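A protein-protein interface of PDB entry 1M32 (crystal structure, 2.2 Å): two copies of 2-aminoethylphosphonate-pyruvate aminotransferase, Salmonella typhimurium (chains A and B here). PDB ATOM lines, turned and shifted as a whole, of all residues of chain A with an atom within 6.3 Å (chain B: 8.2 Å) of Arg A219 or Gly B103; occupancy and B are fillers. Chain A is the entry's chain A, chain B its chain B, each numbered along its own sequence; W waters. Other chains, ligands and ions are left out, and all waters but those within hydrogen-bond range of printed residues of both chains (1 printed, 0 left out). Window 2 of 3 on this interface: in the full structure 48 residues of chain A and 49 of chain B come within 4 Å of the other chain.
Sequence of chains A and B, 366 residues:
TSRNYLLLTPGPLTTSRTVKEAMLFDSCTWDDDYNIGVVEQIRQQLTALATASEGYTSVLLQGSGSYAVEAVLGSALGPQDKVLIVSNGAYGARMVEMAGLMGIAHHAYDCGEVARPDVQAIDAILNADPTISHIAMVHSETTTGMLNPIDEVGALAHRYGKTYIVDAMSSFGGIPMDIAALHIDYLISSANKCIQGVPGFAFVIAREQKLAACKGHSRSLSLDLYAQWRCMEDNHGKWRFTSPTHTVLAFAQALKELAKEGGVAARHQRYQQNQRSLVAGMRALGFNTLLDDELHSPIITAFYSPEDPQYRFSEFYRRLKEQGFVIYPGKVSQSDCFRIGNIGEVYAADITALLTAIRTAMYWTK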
ATOM      1  N   GLY A  74     -38.489 -25.739  25.507  1.00  0.00           N
ATOM      2  CA  GLY A  74     -37.200 -25.393  26.073  1.00  0.00           C
ATOM      3  C   GLY A  74     -36.885 -26.058  27.401  1.00  0.00           C
ATOM      4  O   GLY A  74     -35.724 -26.095  27.807  1.00  0.00           O
ATOM      5  N   MET A 102     -35.078 -21.284  18.711  1.00  0.00           N
ATOM      6  CA  MET A 102     -34.394 -21.737  19.916  1.00  0.00           C
ATOM      7  C   MET A 102     -33.225 -22.685  19.644  1.00  0.00           C
ATOM      8  O   MET A 102     -32.507 -23.070  20.565  1.00  0.00           O
ATOM      9  CB  MET A 102     -35.414 -22.409  20.846  1.00  0.00           C
ATOM     10  CG  MET A 102     -36.609 -21.518  21.193  1.00  0.00           C
ATOM     11  SD  MET A 102     -38.094 -22.434  21.735  1.00  0.00           S
ATOM     12  CE  MET A 102     -37.711 -22.712  23.493  1.00  0.00           C
ATOM     13  N   GLY A 216     -32.267 -27.490  34.687  1.00  0.00           N
ATOM     14  CA  GLY A 216     -31.181 -26.983  33.867  1.00  0.00           C
ATOM     15  C   GLY A 216     -31.408 -26.981  32.366  1.00  0.00           C
ATOM     16  O   GLY A 216     -30.574 -26.467  31.623  1.00  0.00           O
ATOM     17  N   HIS A 217     -32.520 -27.554  31.910  1.00  0.00           N
ATOM     18  CA  HIS A 217     -32.814 -27.594  30.481  1.00  0.00           C
ATOM     19  C   HIS A 217     -33.107 -26.224  29.861  1.00  0.00           C
ATOM     20  O   HIS A 217     -32.614 -25.910  28.778  1.00  0.00           O
ATOM     21  CB  HIS A 217     -34.007 -28.511  30.196  1.00  0.00           C
ATOM     22  CG  HIS A 217     -33.679 -29.972  30.239  1.00  0.00           C
ATOM     23  ND1 HIS A 217     -34.623 -30.950  30.013  1.00  0.00           N
ATOM     24  CD2 HIS A 217     -32.514 -30.620  30.481  1.00  0.00           C
ATOM     25  CE1 HIS A 217     -34.055 -32.138  30.114  1.00  0.00           C
ATOM     26  NE2 HIS A 217     -32.776 -31.967  30.397  1.00  0.00           N
ATOM     27  N   SER A 218     -33.910 -25.413  30.546  1.00  0.00           N
ATOM     28  CA  SER A 218     -34.285 -24.104  30.020  1.00  0.00           C
ATOM     29  C   SER A 218     -33.198 -23.040  30.069  1.00  0.00           C
ATOM     30  O   SER A 218     -32.502 -22.889  31.075  1.00  0.00           O
ATOM     31  CB  SER A 218     -35.519 -23.567  30.753  1.00  0.00           C
ATOM     32  OG  SER A 218     -35.909 -22.310  30.219  1.00  0.00           O
ATOM     33  N   ARG A 219     -33.066 -22.299  28.973  1.00  0.00           N
ATOM     34  CA  ARG A 219     -32.100 -21.213  28.901  1.00  0.00           C
ATOM     35  C   ARG A 219     -32.848 -19.927  29.256  1.00  0.00           C
ATOM     36  O   ARG A 219     -32.268 -18.847  29.318  1.00  0.00           O
ATOM     37  CB  ARG A 219     -31.496 -21.106  27.495  1.00  0.00           C
ATOM     38  CG  ARG A 219     -30.786 -22.372  27.015  1.00  0.00           C
ATOM     39  CD  ARG A 219     -29.760 -22.062  25.920  1.00  0.00           C
ATOM     40  NE  ARG A 219     -28.533 -21.522  26.496  1.00  0.00           N
ATOM     41  CZ  ARG A 219     -27.848 -20.501  25.990  1.00  0.00           C
ATOM     42  NH1 ARG A 219     -28.268 -19.895  24.885  1.00  0.00           N
ATOM     43  NH2 ARG A 219     -26.745 -20.078  26.598  1.00  0.00           N
ATOM     44  N   SER A 220     -34.151 -20.064  29.486  1.00  0.00           N
ATOM     45  CA  SER A 220     -35.001 -18.944  29.863  1.00  0.00           C
ATOM     46  C   SER A 220     -35.415 -19.082  31.323  1.00  0.00           C
ATOM     47  O   SER A 220     -35.929 -20.126  31.735  1.00  0.00           O
ATOM     48  CB  SER A 220     -36.257 -18.907  28.987  1.00  0.00           C
ATOM     49  OG  SER A 220     -37.189 -17.942  29.463  1.00  0.00           O
ATOM     50  N   LEU A 221     -35.185 -18.036  32.109  1.00  0.00           N
ATOM     51  CA  LEU A 221     -35.567 -18.070  33.515  1.00  0.00           C
ATOM     52  C   LEU A 221     -37.090 -18.004  33.580  1.00  0.00           C
ATOM     53  O   LEU A 221     -37.738 -18.824  34.234  1.00  0.00           O
ATOM     54  CB  LEU A 221     -34.966 -16.875  34.268  1.00  0.00           C
ATOM     55  CG  LEU A 221     -35.312 -16.761  35.761  1.00  0.00           C
ATOM     56  CD1 LEU A 221     -34.798 -17.988  36.502  1.00  0.00           C
ATOM     57  CD2 LEU A 221     -34.696 -15.490  36.348  1.00  0.00           C
ATOM     58  N   GLU B  70     -36.573  -9.805  30.853  1.00  0.00           N
ATOM     59  CA  GLU B  70     -35.917 -10.820  30.042  1.00  0.00           C
ATOM     60  C   GLU B  70     -36.044 -10.489  28.556  1.00  0.00           C
ATOM     61  O   GLU B  70     -35.092 -10.659  27.796  1.00  0.00           O
ATOM     62  CB  GLU B  70     -36.515 -12.203  30.319  1.00  0.00           C
ATOM     63  CG  GLU B  70     -35.676 -13.341  29.753  1.00  0.00           C
ATOM     64  CD  GLU B  70     -36.159 -14.709  30.196  1.00  0.00           C
ATOM     65  OE1 GLU B  70     -36.392 -14.903  31.406  1.00  0.00           O
ATOM     66  OE2 GLU B  70     -36.297 -15.597  29.333  1.00  0.00           O
ATOM     67  N   GLY B  78     -27.337  -7.020  20.660  1.00  0.00           N
ATOM     68  CA  GLY B  78     -26.868  -7.668  19.453  1.00  0.00           C
ATOM     69  C   GLY B  78     -25.847  -8.740  19.798  1.00  0.00           C
ATOM     70  O   GLY B  78     -25.541  -8.946  20.975  1.00  0.00           O
ATOM     71  N   PRO B  79     -25.283  -9.424  18.791  1.00  0.00           N
ATOM     72  CA  PRO B  79     -24.290 -10.487  18.983  1.00  0.00           C
ATOM     73  C   PRO B  79     -23.000 -10.075  19.697  1.00  0.00           C
ATOM     74  O   PRO B  79     -22.528 -10.792  20.580  1.00  0.00           O
ATOM     75  CB  PRO B  79     -24.037 -10.975  17.559  1.00  0.00           C
ATOM     76  CG  PRO B  79     -24.195  -9.721  16.755  1.00  0.00           C
ATOM     77  CD  PRO B  79     -25.445  -9.114  17.359  1.00  0.00           C
ATOM     78  N   ASP B  81     -22.679  -7.367  21.527  1.00  0.00           N
ATOM     79  CA  ASP B  81     -22.998  -6.464  22.625  1.00  0.00           C
ATOM     80  C   ASP B  81     -22.680  -7.058  23.990  1.00  0.00           C
ATOM     81  O   ASP B  81     -22.576  -8.277  24.144  1.00  0.00           O
ATOM     82  CB  ASP B  81     -24.470  -6.060  22.559  1.00  0.00           C
ATOM     83  CG  ASP B  81     -24.754  -5.089  21.426  1.00  0.00           C
ATOM     84  OD1 ASP B  81     -25.940  -4.878  21.104  1.00  0.00           O
ATOM     85  OD2 ASP B  81     -23.788  -4.530  20.862  1.00  0.00           O
ATOM     86  N   VAL B  96     -28.609 -10.477  36.325  1.00  0.00           N
ATOM     87  CA  VAL B  96     -27.320 -11.143  36.162  1.00  0.00           C
ATOM     88  C   VAL B  96     -27.602 -12.625  35.950  1.00  0.00           C
ATOM     89  O   VAL B  96     -26.991 -13.278  35.105  1.00  0.00           O
ATOM     90  CB  VAL B  96     -26.426 -10.966  37.409  1.00  0.00           C
ATOM     91  CG1 VAL B  96     -25.179 -11.837  37.290  1.00  0.00           C
ATOM     92  CG2 VAL B  96     -26.033  -9.504  37.565  1.00  0.00           C
ATOM     93  N   GLU B  97     -28.545 -13.147  36.727  1.00  0.00           N
ATOM     94  CA  GLU B  97     -28.930 -14.545  36.621  1.00  0.00           C
ATOM     95  C   GLU B  97     -29.430 -14.826  35.206  1.00  0.00           C
ATOM     96  O   GLU B  97     -29.021 -15.802  34.580  1.00  0.00           O
ATOM     97  CB  GLU B  97     -30.032 -14.857  37.631  1.00  0.00           C
ATOM     98  CG  GLU B  97     -30.516 -16.290  37.586  1.00  0.00           C
ATOM     99  CD  GLU B  97     -31.643 -16.545  38.559  1.00  0.00           C
ATOM    100  OE1 GLU B  97     -32.081 -17.707  38.665  1.00  0.00           O
ATOM    101  OE2 GLU B  97     -32.097 -15.585  39.219  1.00  0.00           O
ATOM    102  N   MET B  98     -30.311 -13.962  34.706  1.00  0.00           N
ATOM    103  CA  MET B  98     -30.854 -14.120  33.360  1.00  0.00           C
ATOM    104  C   MET B  98     -29.743 -14.065  32.315  1.00  0.00           C
ATOM    105  O   MET B  98     -29.699 -14.889  31.405  1.00  0.00           O
ATOM    106  CB  MET B  98     -31.881 -13.023  33.052  1.00  0.00           C
ATOM    107  CG  MET B  98     -33.145 -13.062  33.899  1.00  0.00           C
ATOM    108  SD  MET B  98     -34.252 -11.654  33.554  1.00  0.00           S
ATOM    109  CE  MET B  98     -35.846 -12.350  34.092  1.00  0.00           C
ATOM    110  N   ALA B  99     -28.854 -13.084  32.446  1.00  0.00           N
ATOM    111  CA  ALA B  99     -27.750 -12.924  31.504  1.00  0.00           C
ATOM    112  C   ALA B  99     -26.911 -14.194  31.445  1.00  0.00           C
ATOM    113  O   ALA B  99     -26.466 -14.605  30.373  1.00  0.00           O
ATOM    114  CB  ALA B  99     -26.878 -11.734  31.909  1.00  0.00           C
ATOM    115  N   GLY B 100     -26.705 -14.811  32.605  1.00  0.00           N
ATOM    116  CA  GLY B 100     -25.925 -16.033  32.674  1.00  0.00           C
ATOM    117  C   GLY B 100     -26.586 -17.182  31.935  1.00  0.00           C
ATOM    118  O   GLY B 100     -25.954 -17.838  31.113  1.00  0.00           O
ATOM    119  N   LEU B 101     -27.861 -17.421  32.228  1.00  0.00           N
ATOM    120  CA  LEU B 101     -28.624 -18.494  31.587  1.00  0.00           C
ATOM    121  C   LEU B 101     -28.700 -18.344  30.074  1.00  0.00           C
ATOM    122  O   LEU B 101     -28.647 -19.330  29.337  1.00  0.00           O
ATOM    123  CB  LEU B 101     -30.056 -18.526  32.133  1.00  0.00           C
ATOM    124  CG  LEU B 101     -30.324 -19.153  33.500  1.00  0.00           C
ATOM    125  CD1 LEU B 101     -31.727 -18.783  33.969  1.00  0.00           C
ATOM    126  CD2 LEU B 101     -30.168 -20.669  33.403  1.00  0.00           C
ATOM    127  N   MET B 102     -28.841 -17.104  29.625  1.00  0.00           N
ATOM    128  CA  MET B 102     -28.971 -16.794  28.208  1.00  0.00           C
ATOM    129  C   MET B 102     -27.634 -16.690  27.478  1.00  0.00           C
ATOM    130  O   MET B 102     -27.604 -16.517  26.262  1.00  0.00           O
ATOM    131  CB  MET B 102     -29.763 -15.488  28.054  1.00  0.00           C
ATOM    132  CG  MET B 102     -31.146 -15.531  28.719  1.00  0.00           C
ATOM    133  SD  MET B 102     -31.874 -13.896  29.130  1.00  0.00           S
ATOM    134  CE  MET B 102     -32.697 -13.478  27.572  1.00  0.00           C
ATOM    135  N   GLY B 103     -26.534 -16.807  28.215  1.00  0.00           N
ATOM    136  CA  GLY B 103     -25.221 -16.715  27.600  1.00  0.00           C
ATOM    137  C   GLY B 103     -24.925 -15.328  27.055  1.00  0.00           C
ATOM    138  O   GLY B 103     -24.208 -15.174  26.064  1.00  0.00           O
ATOM    139  N   ILE B 104     -25.479 -14.313  27.708  1.00  0.00           N
ATOM    140  CA  ILE B 104     -25.277 -12.932  27.288  1.00  0.00           C
ATOM    141  C   ILE B 104     -24.032 -12.338  27.940  1.00  0.00           C
ATOM    142  O   ILE B 104     -23.890 -12.364  29.164  1.00  0.00           O
ATOM    143  CB  ILE B 104     -26.503 -12.065  27.660  1.00  0.00           C
ATOM    144  CG1 ILE B 104     -27.719 -12.520  26.849  1.00  0.00           C
ATOM    145  CG2 ILE B 104     -26.206 -10.585  27.406  1.00  0.00           C
ATOM    146  CD1 ILE B 104     -29.013 -11.824  27.236  1.00  0.00           C
ATOM    147  N   ALA B 105     -23.126 -11.811  27.122  1.00  0.00           N
ATOM    148  CA  ALA B 105     -21.909 -11.202  27.646  1.00  0.00           C
ATOM    149  C   ALA B 105     -22.334 -10.080  28.590  1.00  0.00           C
ATOM    150  O   ALA B 105     -23.221  -9.290  28.266  1.00  0.00           O
ATOM    151  CB  ALA B 105     -21.056 -10.647  26.503  1.00  0.00           C
ATOM    152  N   HIS B 106     -21.708 -10.010  29.757  1.00  0.00           N
ATOM    153  CA  HIS B 106     -22.071  -8.988  30.723  1.00  0.00           C
ATOM    154  C   HIS B 106     -20.964  -8.723  31.725  1.00  0.00           C
ATOM    155  O   HIS B 106     -20.012  -9.491  31.845  1.00  0.00           O
ATOM    156  CB  HIS B 106     -23.318  -9.425  31.494  1.00  0.00           C
ATOM    157  CG  HIS B 106     -23.123 -10.692  32.270  1.00  0.00           C
ATOM    158  ND1 HIS B 106     -23.048 -11.931  31.667  1.00  0.00           N
ATOM    159  CD2 HIS B 106     -22.933 -10.907  33.593  1.00  0.00           C
ATOM    160  CE1 HIS B 106     -22.820 -12.853  32.585  1.00  0.00           C
ATOM    161  NE2 HIS B 106     -22.746 -12.259  33.763  1.00  0.00           N
ATOM    162  N   ARG B 219     -34.107 -14.846  20.634  1.00  0.00           N
ATOM    163  CA  ARG B 219     -34.083 -16.272  20.332  1.00  0.00           C
ATOM    164  C   ARG B 219     -35.383 -16.857  20.869  1.00  0.00           C
ATOM    165  O   ARG B 219     -35.635 -18.053  20.754  1.00  0.00           O
ATOM    166  CB  ARG B 219     -32.904 -16.969  21.018  1.00  0.00           C
ATOM    167  CG  ARG B 219     -31.533 -16.545  20.521  1.00  0.00           C
HETATM  168  O   HOH W   1     -33.131 -16.277  31.324  1.00  0.00           O
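Met A102 touches Arg B219, and with the chains exchanged Arg A219 touches Met B102.
2 positions are printed for both chains.
Of the 10 pairs that touch across the chains among the printed residues, 2 have their exchanged pair printed and touching as well.
Of the printed residues of chain B, Met A102 touches Arg B219.
Arg A219 touches just these residues of chain B: Leu B101 (3.4 Å), Met B102 (3.6 Å) and Gly B103 (3.7 Å).
Printed residues of chain A within 4 Å of Glu B70: Ser A220 (2.5 Å) and Leu A221 (3.4 Å).
Of the printed residues of chain A, Glu B97 touches Leu A221.
Printed residues of chain A within 4 Å of Leu B101: Ser A218 (3.97 Å), Arg A219 (3.4 Å) and Leu A221 (3.8 Å).
Of the printed residues of chain A, Met B102 touches Arg A219.
Of chain A, only Arg A219 (3.7 Å) comes within 4 Å of Gly B103.
The nearest printed residue of chain A that does not touch Gly B103 is Ser A220 (8.4 Å).
Hydrophobic or aromatic side chains of chain B that line the printed part of chain A: Met B98, Leu B101 and Met B102.
Of the 8 printed residues of chain A, 5 touch a printed residue of chain B.
Hydrophobic or aromatic side chains of chain A within 4 Å of the printed part of chain B: Met A102 and Leu A221.
Along chain A the printed residues that touch a printed residue of chain B span positions 102 to 221.
Water W1 lies within hydrogen-bond range of the backbone NH of Leu A221 (2.8 Å), the backbone carbonyl oxygen of Arg A219 (3.4 Å) and the side-chain sulfur of Met B102 (3.5 Å).
O of Gly A74 sits close to N of Ser A218 (3.4 Å).
OG of Ser A218 lies within hydrogen-bond range of O of Ser A220.
N of Leu A221 is in hydrogen-bond range of OE1 of Glu B70, at 3.4 Å.
OE2 of Glu B70 is in hydrogen-bond range of OG of Ser A220 (2.5 Å).
O of Leu B101 sits at hydrogen-bond distance from NH2 of Arg A219 (3.4 Å).
Among the printed residues, pairs that only touch across the chains: Leu A221 with Glu B97, Arg A219 with Met B102, Met A102 with Arg B219, Arg A219 with Gly B103, Leu A221 with Leu B101, Leu A221 with Met B98 and Ser A218 with Leu B101.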
